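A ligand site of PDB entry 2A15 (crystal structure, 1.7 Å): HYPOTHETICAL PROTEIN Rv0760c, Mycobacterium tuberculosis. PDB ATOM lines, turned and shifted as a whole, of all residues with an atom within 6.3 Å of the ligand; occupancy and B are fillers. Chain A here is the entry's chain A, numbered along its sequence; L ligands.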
ATOM      1  N   ALA A  12      10.257  38.132  20.096  1.00  0.00           N
ATOM      2  CA  ALA A  12      10.768  36.765  20.365  1.00  0.00           C
ATOM      3  C   ALA A  12      10.569  35.893  19.134  1.00  0.00           C
ATOM      4  O   ALA A  12      11.497  35.202  18.723  1.00  0.00           O
ATOM      5  CB  ALA A  12      10.162  36.169  21.589  1.00  0.00           C
ATOM      6  N   SER A  13       9.382  35.939  18.512  1.00  0.00           N
ATOM      7  CA  SER A  13       9.191  35.093  17.335  1.00  0.00           C
ATOM      8  C   SER A  13      10.033  35.535  16.134  1.00  0.00           C
ATOM      9  O   SER A  13      10.687  34.702  15.500  1.00  0.00           O
ATOM     10  CB  SER A  13       7.695  35.033  16.985  1.00  0.00           C
ATOM     11  OG  SER A  13       7.231  36.238  16.403  1.00  0.00           O
ATOM     12  N   SER A  16      13.565  34.559  16.790  1.00  0.00           N
ATOM     13  CA  SER A  16      13.811  33.142  16.656  1.00  0.00           C
ATOM     14  C   SER A  16      14.114  32.751  15.195  1.00  0.00           C
ATOM     15  O   SER A  16      15.063  31.987  14.957  1.00  0.00           O
ATOM     16  CB  SER A  16      12.659  32.326  17.279  1.00  0.00           C
ATOM     17  OG  SER A  16      11.511  32.328  16.420  1.00  0.00           O
ATOM     18  N   TRP A  17      13.391  33.321  14.220  1.00  0.00           N
ATOM     19  CA  TRP A  17      13.674  33.004  12.809  1.00  0.00           C
ATOM     20  C   TRP A  17      14.959  33.654  12.315  1.00  0.00           C
ATOM     21  O   TRP A  17      15.685  33.060  11.538  1.00  0.00           O
ATOM     22  CB  TRP A  17      12.582  33.622  11.896  1.00  0.00           C
ATOM     23  CG  TRP A  17      11.175  33.496  12.403  1.00  0.00           C
ATOM     24  CD1 TRP A  17      10.661  32.477  13.127  1.00  0.00           C
ATOM     25  CD2 TRP A  17      10.103  34.450  12.229  1.00  0.00           C
ATOM     26  NE1 TRP A  17       9.340  32.697  13.396  1.00  0.00           N
ATOM     27  CE2 TRP A  17       8.962  33.906  12.855  1.00  0.00           C
ATOM     28  CE3 TRP A  17       9.989  35.674  11.545  1.00  0.00           C
ATOM     29  CZ2 TRP A  17       7.727  34.563  12.870  1.00  0.00           C
ATOM     30  CZ3 TRP A  17       8.753  36.348  11.574  1.00  0.00           C
ATOM     31  CH2 TRP A  17       7.644  35.785  12.245  1.00  0.00           C
ATOM     32  N   VAL A  20      17.617  31.403  13.408  1.00  0.00           N
ATOM     33  CA  VAL A  20      17.649  30.259  12.512  1.00  0.00           C
ATOM     34  C   VAL A  20      18.394  30.636  11.230  1.00  0.00           C
ATOM     35  O   VAL A  20      19.302  29.914  10.792  1.00  0.00           O
ATOM     36  CB  VAL A  20      16.222  29.658  12.209  1.00  0.00           C
ATOM     37  CG1 VAL A  20      16.292  28.607  11.068  1.00  0.00           C
ATOM     38  CG2 VAL A  20      15.655  28.999  13.484  1.00  0.00           C
ATOM     39  N   TRP A  28      19.752  31.667  19.411  1.00  0.00           N
ATOM     40  CA  TRP A  28      18.429  30.992  19.456  1.00  0.00           C
ATOM     41  C   TRP A  28      18.065  30.490  20.868  1.00  0.00           C
ATOM     42  O   TRP A  28      16.979  30.789  21.386  1.00  0.00           O
ATOM     43  CB  TRP A  28      18.429  29.856  18.400  1.00  0.00           C
ATOM     44  CG  TRP A  28      17.052  29.259  18.088  1.00  0.00           C
ATOM     45  CD1 TRP A  28      16.076  29.772  17.253  1.00  0.00           C
ATOM     46  CD2 TRP A  28      16.542  28.044  18.606  1.00  0.00           C
ATOM     47  NE1 TRP A  28      14.973  28.909  17.229  1.00  0.00           N
ATOM     48  CE2 TRP A  28      15.239  27.861  18.052  1.00  0.00           C
ATOM     49  CE3 TRP A  28      17.064  27.073  19.486  1.00  0.00           C
ATOM     50  CZ2 TRP A  28      14.462  26.724  18.349  1.00  0.00           C
ATOM     51  CZ3 TRP A  28      16.286  25.959  19.776  1.00  0.00           C
ATOM     52  CH2 TRP A  28      14.992  25.789  19.206  1.00  0.00           C
ATOM     53  N   MET A  32      15.053  31.502  24.778  1.00  0.00           N
ATOM     54  CA  MET A  32      14.209  30.501  25.419  1.00  0.00           C
ATOM     55  C   MET A  32      14.266  30.598  26.911  1.00  0.00           C
ATOM     56  O   MET A  32      15.339  30.770  27.501  1.00  0.00           O
ATOM     57  CB  MET A  32      14.625  29.074  25.026  1.00  0.00           C
ATOM     58  CG  MET A  32      14.780  28.873  23.544  1.00  0.00           C
ATOM     59  SD  MET A  32      13.207  29.083  22.696  1.00  0.00           S
ATOM     60  CE  MET A  32      13.810  29.111  21.021  1.00  0.00           C
ATOM     61  N   ASP A  40       6.959  21.083  18.046  1.00  0.00           N
ATOM     62  CA  ASP A  40       6.994  21.343  16.612  1.00  0.00           C
ATOM     63  C   ASP A  40       7.068  20.012  15.865  1.00  0.00           C
ATOM     64  O   ASP A  40       8.160  19.475  15.629  1.00  0.00           O
ATOM     65  CB  ASP A  40       8.246  22.193  16.288  1.00  0.00           C
ATOM     66  CG  ASP A  40       8.532  22.293  14.782  1.00  0.00           C
ATOM     67  OD1 ASP A  40       7.574  22.348  13.988  1.00  0.00           O
ATOM     68  OD2 ASP A  40       9.726  22.276  14.393  1.00  0.00           O
ATOM     69  N   PHE A  63      17.595  19.541  19.747  1.00  0.00           N
ATOM     70  CA  PHE A  63      16.587  19.775  18.685  1.00  0.00           C
ATOM     71  C   PHE A  63      17.072  20.749  17.614  1.00  0.00           C
ATOM     72  O   PHE A  63      16.922  20.488  16.426  1.00  0.00           O
ATOM     73  CB  PHE A  63      15.259  20.237  19.335  1.00  0.00           C
ATOM     74  CG  PHE A  63      14.200  20.688  18.359  1.00  0.00           C
ATOM     75  CD1 PHE A  63      13.287  19.765  17.829  1.00  0.00           C
ATOM     76  CD2 PHE A  63      14.108  22.006  17.962  1.00  0.00           C
ATOM     77  CE1 PHE A  63      12.313  20.182  16.920  1.00  0.00           C
ATOM     78  CE2 PHE A  63      13.133  22.413  17.051  1.00  0.00           C
ATOM     79  CZ  PHE A  63      12.234  21.484  16.536  1.00  0.00           C
ATOM     80  N   HIS A  67      17.282  19.064  14.035  1.00  0.00           N
ATOM     81  CA  HIS A  67      16.097  19.473  13.284  1.00  0.00           C
ATOM     82  C   HIS A  67      16.000  20.923  12.799  1.00  0.00           C
ATOM     83  O   HIS A  67      14.974  21.331  12.178  1.00  0.00           O
ATOM     84  CB  HIS A  67      14.837  19.097  14.102  1.00  0.00           C
ATOM     85  CG  HIS A  67      14.780  17.643  14.436  1.00  0.00           C
ATOM     86  ND1 HIS A  67      14.709  16.653  13.466  1.00  0.00           N
ATOM     87  CD2 HIS A  67      14.791  17.001  15.625  1.00  0.00           C
ATOM     88  CE1 HIS A  67      14.669  15.470  14.064  1.00  0.00           C
ATOM     89  NE2 HIS A  67      14.699  15.659  15.359  1.00  0.00           N
ATOM     90  N   ILE A  68      17.057  21.716  13.023  1.00  0.00           N
ATOM     91  CA  ILE A  68      17.136  23.057  12.442  1.00  0.00           C
ATOM     92  C   ILE A  68      18.423  23.200  11.612  1.00  0.00           C
ATOM     93  O   ILE A  68      18.383  23.604  10.463  1.00  0.00           O
ATOM     94  CB  ILE A  68      17.051  24.177  13.533  1.00  0.00           C
ATOM     95  CG1 ILE A  68      15.633  24.153  14.168  1.00  0.00           C
ATOM     96  CG2 ILE A  68      17.288  25.540  12.883  1.00  0.00           C
ATOM     97  CD1 ILE A  68      15.409  25.139  15.336  1.00  0.00           C
ATOM     98  N   LEU A  73      17.146  23.765   7.744  1.00  0.00           N
ATOM     99  CA  LEU A  73      15.805  24.367   7.867  1.00  0.00           C
ATOM    100  C   LEU A  73      15.824  25.855   7.511  1.00  0.00           C
ATOM    101  O   LEU A  73      16.717  26.620   7.978  1.00  0.00           O
ATOM    102  CB  LEU A  73      15.305  24.149   9.294  1.00  0.00           C
ATOM    103  CG  LEU A  73      13.866  24.691   9.505  1.00  0.00           C
ATOM    104  CD1 LEU A  73      12.877  23.749   8.790  1.00  0.00           C
ATOM    105  CD2 LEU A  73      13.557  24.817  11.012  1.00  0.00           C
ATOM    106  N   VAL A  75      12.946  29.145   7.508  1.00  0.00           N
ATOM    107  CA  VAL A  75      11.651  29.544   8.061  1.00  0.00           C
ATOM    108  C   VAL A  75      11.246  30.861   7.416  1.00  0.00           C
ATOM    109  O   VAL A  75      12.007  31.851   7.464  1.00  0.00           O
ATOM    110  CB  VAL A  75      11.733  29.685   9.606  1.00  0.00           C
ATOM    111  CG1 VAL A  75      10.343  30.021  10.181  1.00  0.00           C
ATOM    112  CG2 VAL A  75      12.236  28.411  10.260  1.00  0.00           C
ATOM    113  N   LEU A  93       3.699  30.012   9.022  1.00  0.00           N
ATOM    114  CA  LEU A  93       5.096  29.872   8.569  1.00  0.00           C
ATOM    115  C   LEU A  93       5.207  28.778   7.517  1.00  0.00           C
ATOM    116  O   LEU A  93       4.485  27.769   7.552  1.00  0.00           O
ATOM    117  CB  LEU A  93       6.019  29.511   9.723  1.00  0.00           C
ATOM    118  CG  LEU A  93       6.020  30.343  10.999  1.00  0.00           C
ATOM    119  CD1 LEU A  93       7.037  29.793  11.980  1.00  0.00           C
ATOM    120  CD2 LEU A  93       6.295  31.792  10.620  1.00  0.00           C
ATOM    121  N   LEU A  95       8.032  26.181   6.253  1.00  0.00           N
ATOM    122  CA  LEU A  95       9.297  25.551   6.651  1.00  0.00           C
ATOM    123  C   LEU A  95       9.837  24.764   5.478  1.00  0.00           C
ATOM    124  O   LEU A  95       9.079  24.048   4.826  1.00  0.00           O
ATOM    125  CB  LEU A  95       9.139  24.610   7.847  1.00  0.00           C
ATOM    126  CG  LEU A  95       8.443  25.170   9.103  1.00  0.00           C
ATOM    127  CD1 LEU A  95       8.436  24.076  10.148  1.00  0.00           C
ATOM    128  CD2 LEU A  95       9.067  26.437   9.601  1.00  0.00           C
ATOM    129  N   PHE A 111       1.938  28.434  13.638  1.00  0.00           N
ATOM    130  CA  PHE A 111       2.807  28.298  14.812  1.00  0.00           C
ATOM    131  C   PHE A 111       2.420  29.349  15.850  1.00  0.00           C
ATOM    132  O   PHE A 111       2.283  30.521  15.515  1.00  0.00           O
ATOM    133  CB  PHE A 111       4.277  28.455  14.418  1.00  0.00           C
ATOM    134  CG  PHE A 111       4.774  27.303  13.557  1.00  0.00           C
ATOM    135  CD1 PHE A 111       5.570  26.304  14.100  1.00  0.00           C
ATOM    136  CD2 PHE A 111       4.367  27.241  12.235  1.00  0.00           C
ATOM    137  CE1 PHE A 111       5.973  25.238  13.257  1.00  0.00           C
ATOM    138  CE2 PHE A 111       4.768  26.176  11.425  1.00  0.00           C
ATOM    139  CZ  PHE A 111       5.545  25.206  11.952  1.00  0.00           C
ATOM    140  N   TYR A 113       3.226  31.117  19.661  1.00  0.00           N
ATOM    141  CA  TYR A 113       4.320  31.379  20.592  1.00  0.00           C
ATOM    142  C   TYR A 113       3.760  32.029  21.851  1.00  0.00           C
ATOM    143  O   TYR A 113       2.863  32.864  21.768  1.00  0.00           O
ATOM    144  CB  TYR A 113       5.356  32.360  20.015  1.00  0.00           C
ATOM    145  CG  TYR A 113       6.082  31.877  18.766  1.00  0.00           C
ATOM    146  CD1 TYR A 113       7.463  31.601  18.805  1.00  0.00           C
ATOM    147  CD2 TYR A 113       5.408  31.737  17.550  1.00  0.00           C
ATOM    148  CE1 TYR A 113       8.124  31.178  17.650  1.00  0.00           C
ATOM    149  CE2 TYR A 113       6.068  31.298  16.414  1.00  0.00           C
ATOM    150  CZ  TYR A 113       7.435  31.040  16.472  1.00  0.00           C
ATOM    151  OH  TYR A 113       8.079  30.616  15.331  1.00  0.00           O
ATOM    152  N   MET A 124       6.544  27.084  22.029  1.00  0.00           N
ATOM    153  CA  MET A 124       6.337  27.250  20.598  1.00  0.00           C
ATOM    154  C   MET A 124       5.633  25.978  20.129  1.00  0.00           C
ATOM    155  O   MET A 124       6.107  24.870  20.398  1.00  0.00           O
ATOM    156  CB  MET A 124       7.649  27.446  19.825  1.00  0.00           C
ATOM    157  CG  MET A 124       7.401  27.748  18.346  1.00  0.00           C
ATOM    158  SD  MET A 124       8.926  27.902  17.405  1.00  0.00           S
ATOM    159  CE  MET A 124       9.618  26.272  17.672  1.00  0.00           C
HETATM  160  N1  LIG L   1      11.594  25.719  13.943  1.00  0.00           N
HETATM  161  C1  LIG L   1      11.997  26.861  14.537  1.00  0.00           C
HETATM  162  C2  LIG L   1      11.116  27.961  14.548  1.00  0.00           C
HETATM  163  C3  LIG L   1       9.872  27.874  13.917  1.00  0.00           C
HETATM  164  C4  LIG L   1       9.517  26.676  13.300  1.00  0.00           C
HETATM  165  C5  LIG L   1      10.413  25.596  13.323  1.00  0.00           C
HETATM  166  C6  LIG L   1      11.534  29.244  15.233  1.00  0.00           C
HETATM  167  O1  LIG L   1      12.634  29.281  15.798  1.00  0.00           O
HETATM  168  N2  LIG L   1      10.674  30.277  15.173  1.00  0.00           N
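The indole nitrogen (NE1) of Trp 17 lies close to a nitrogen (N2) of the ligand, at 3.3 Å. CG2 of Val 20 touches O1 of the ligand (3.8 Å). Asp 40 touches the ligand (OD2 to C5, 3.6 Å). Ile 68 touches the ligand. Leu 73 touches the ligand. Leu 93 touches the ligand (CD1 to C3, 3.9 Å). Leu 95 touches the ligand (CD2 to C4, 3.7 Å). Phe 111 touches the ligand (CE1 to C4, 3.8 Å).
An oxygen (O1) of the ligand lies within hydrogen-bond range of the indole nitrogen (NE1) of Trp 28, at 2.8 Å. A nitrogen (N2) of the ligand lies within hydrogen-bond range of the side-chain hydroxyl (OG) of Ser 16, at 2.5 Å. N2 of the ligand sits close to SD of Met 124, at 3.7 Å. The side-chain hydroxyl of Tyr 113 sits at hydrogen-bond distance from a nitrogen (N2) of the ligand.
OH of Tyr 113 sits at hydrogen-bond distance from NE1 of Trp 17 (3.1 Å). The side-chain hydroxyl of Tyr 113 sits close to the side-chain sulfur of Met 124 (3.5 Å). N of Leu 73 lies within hydrogen-bond range of O of Ile 68 (3.0 Å). The indole nitrogen of Trp 17 lies within hydrogen-bond range of the backbone carbonyl oxygen of Ser 13, 3.2 Å away. The side-chain hydroxyl (OG) of Ser 16 lies within hydrogen-bond range of the backbone carbonyl oxygen (O) of Ser 13 (2.7 Å).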
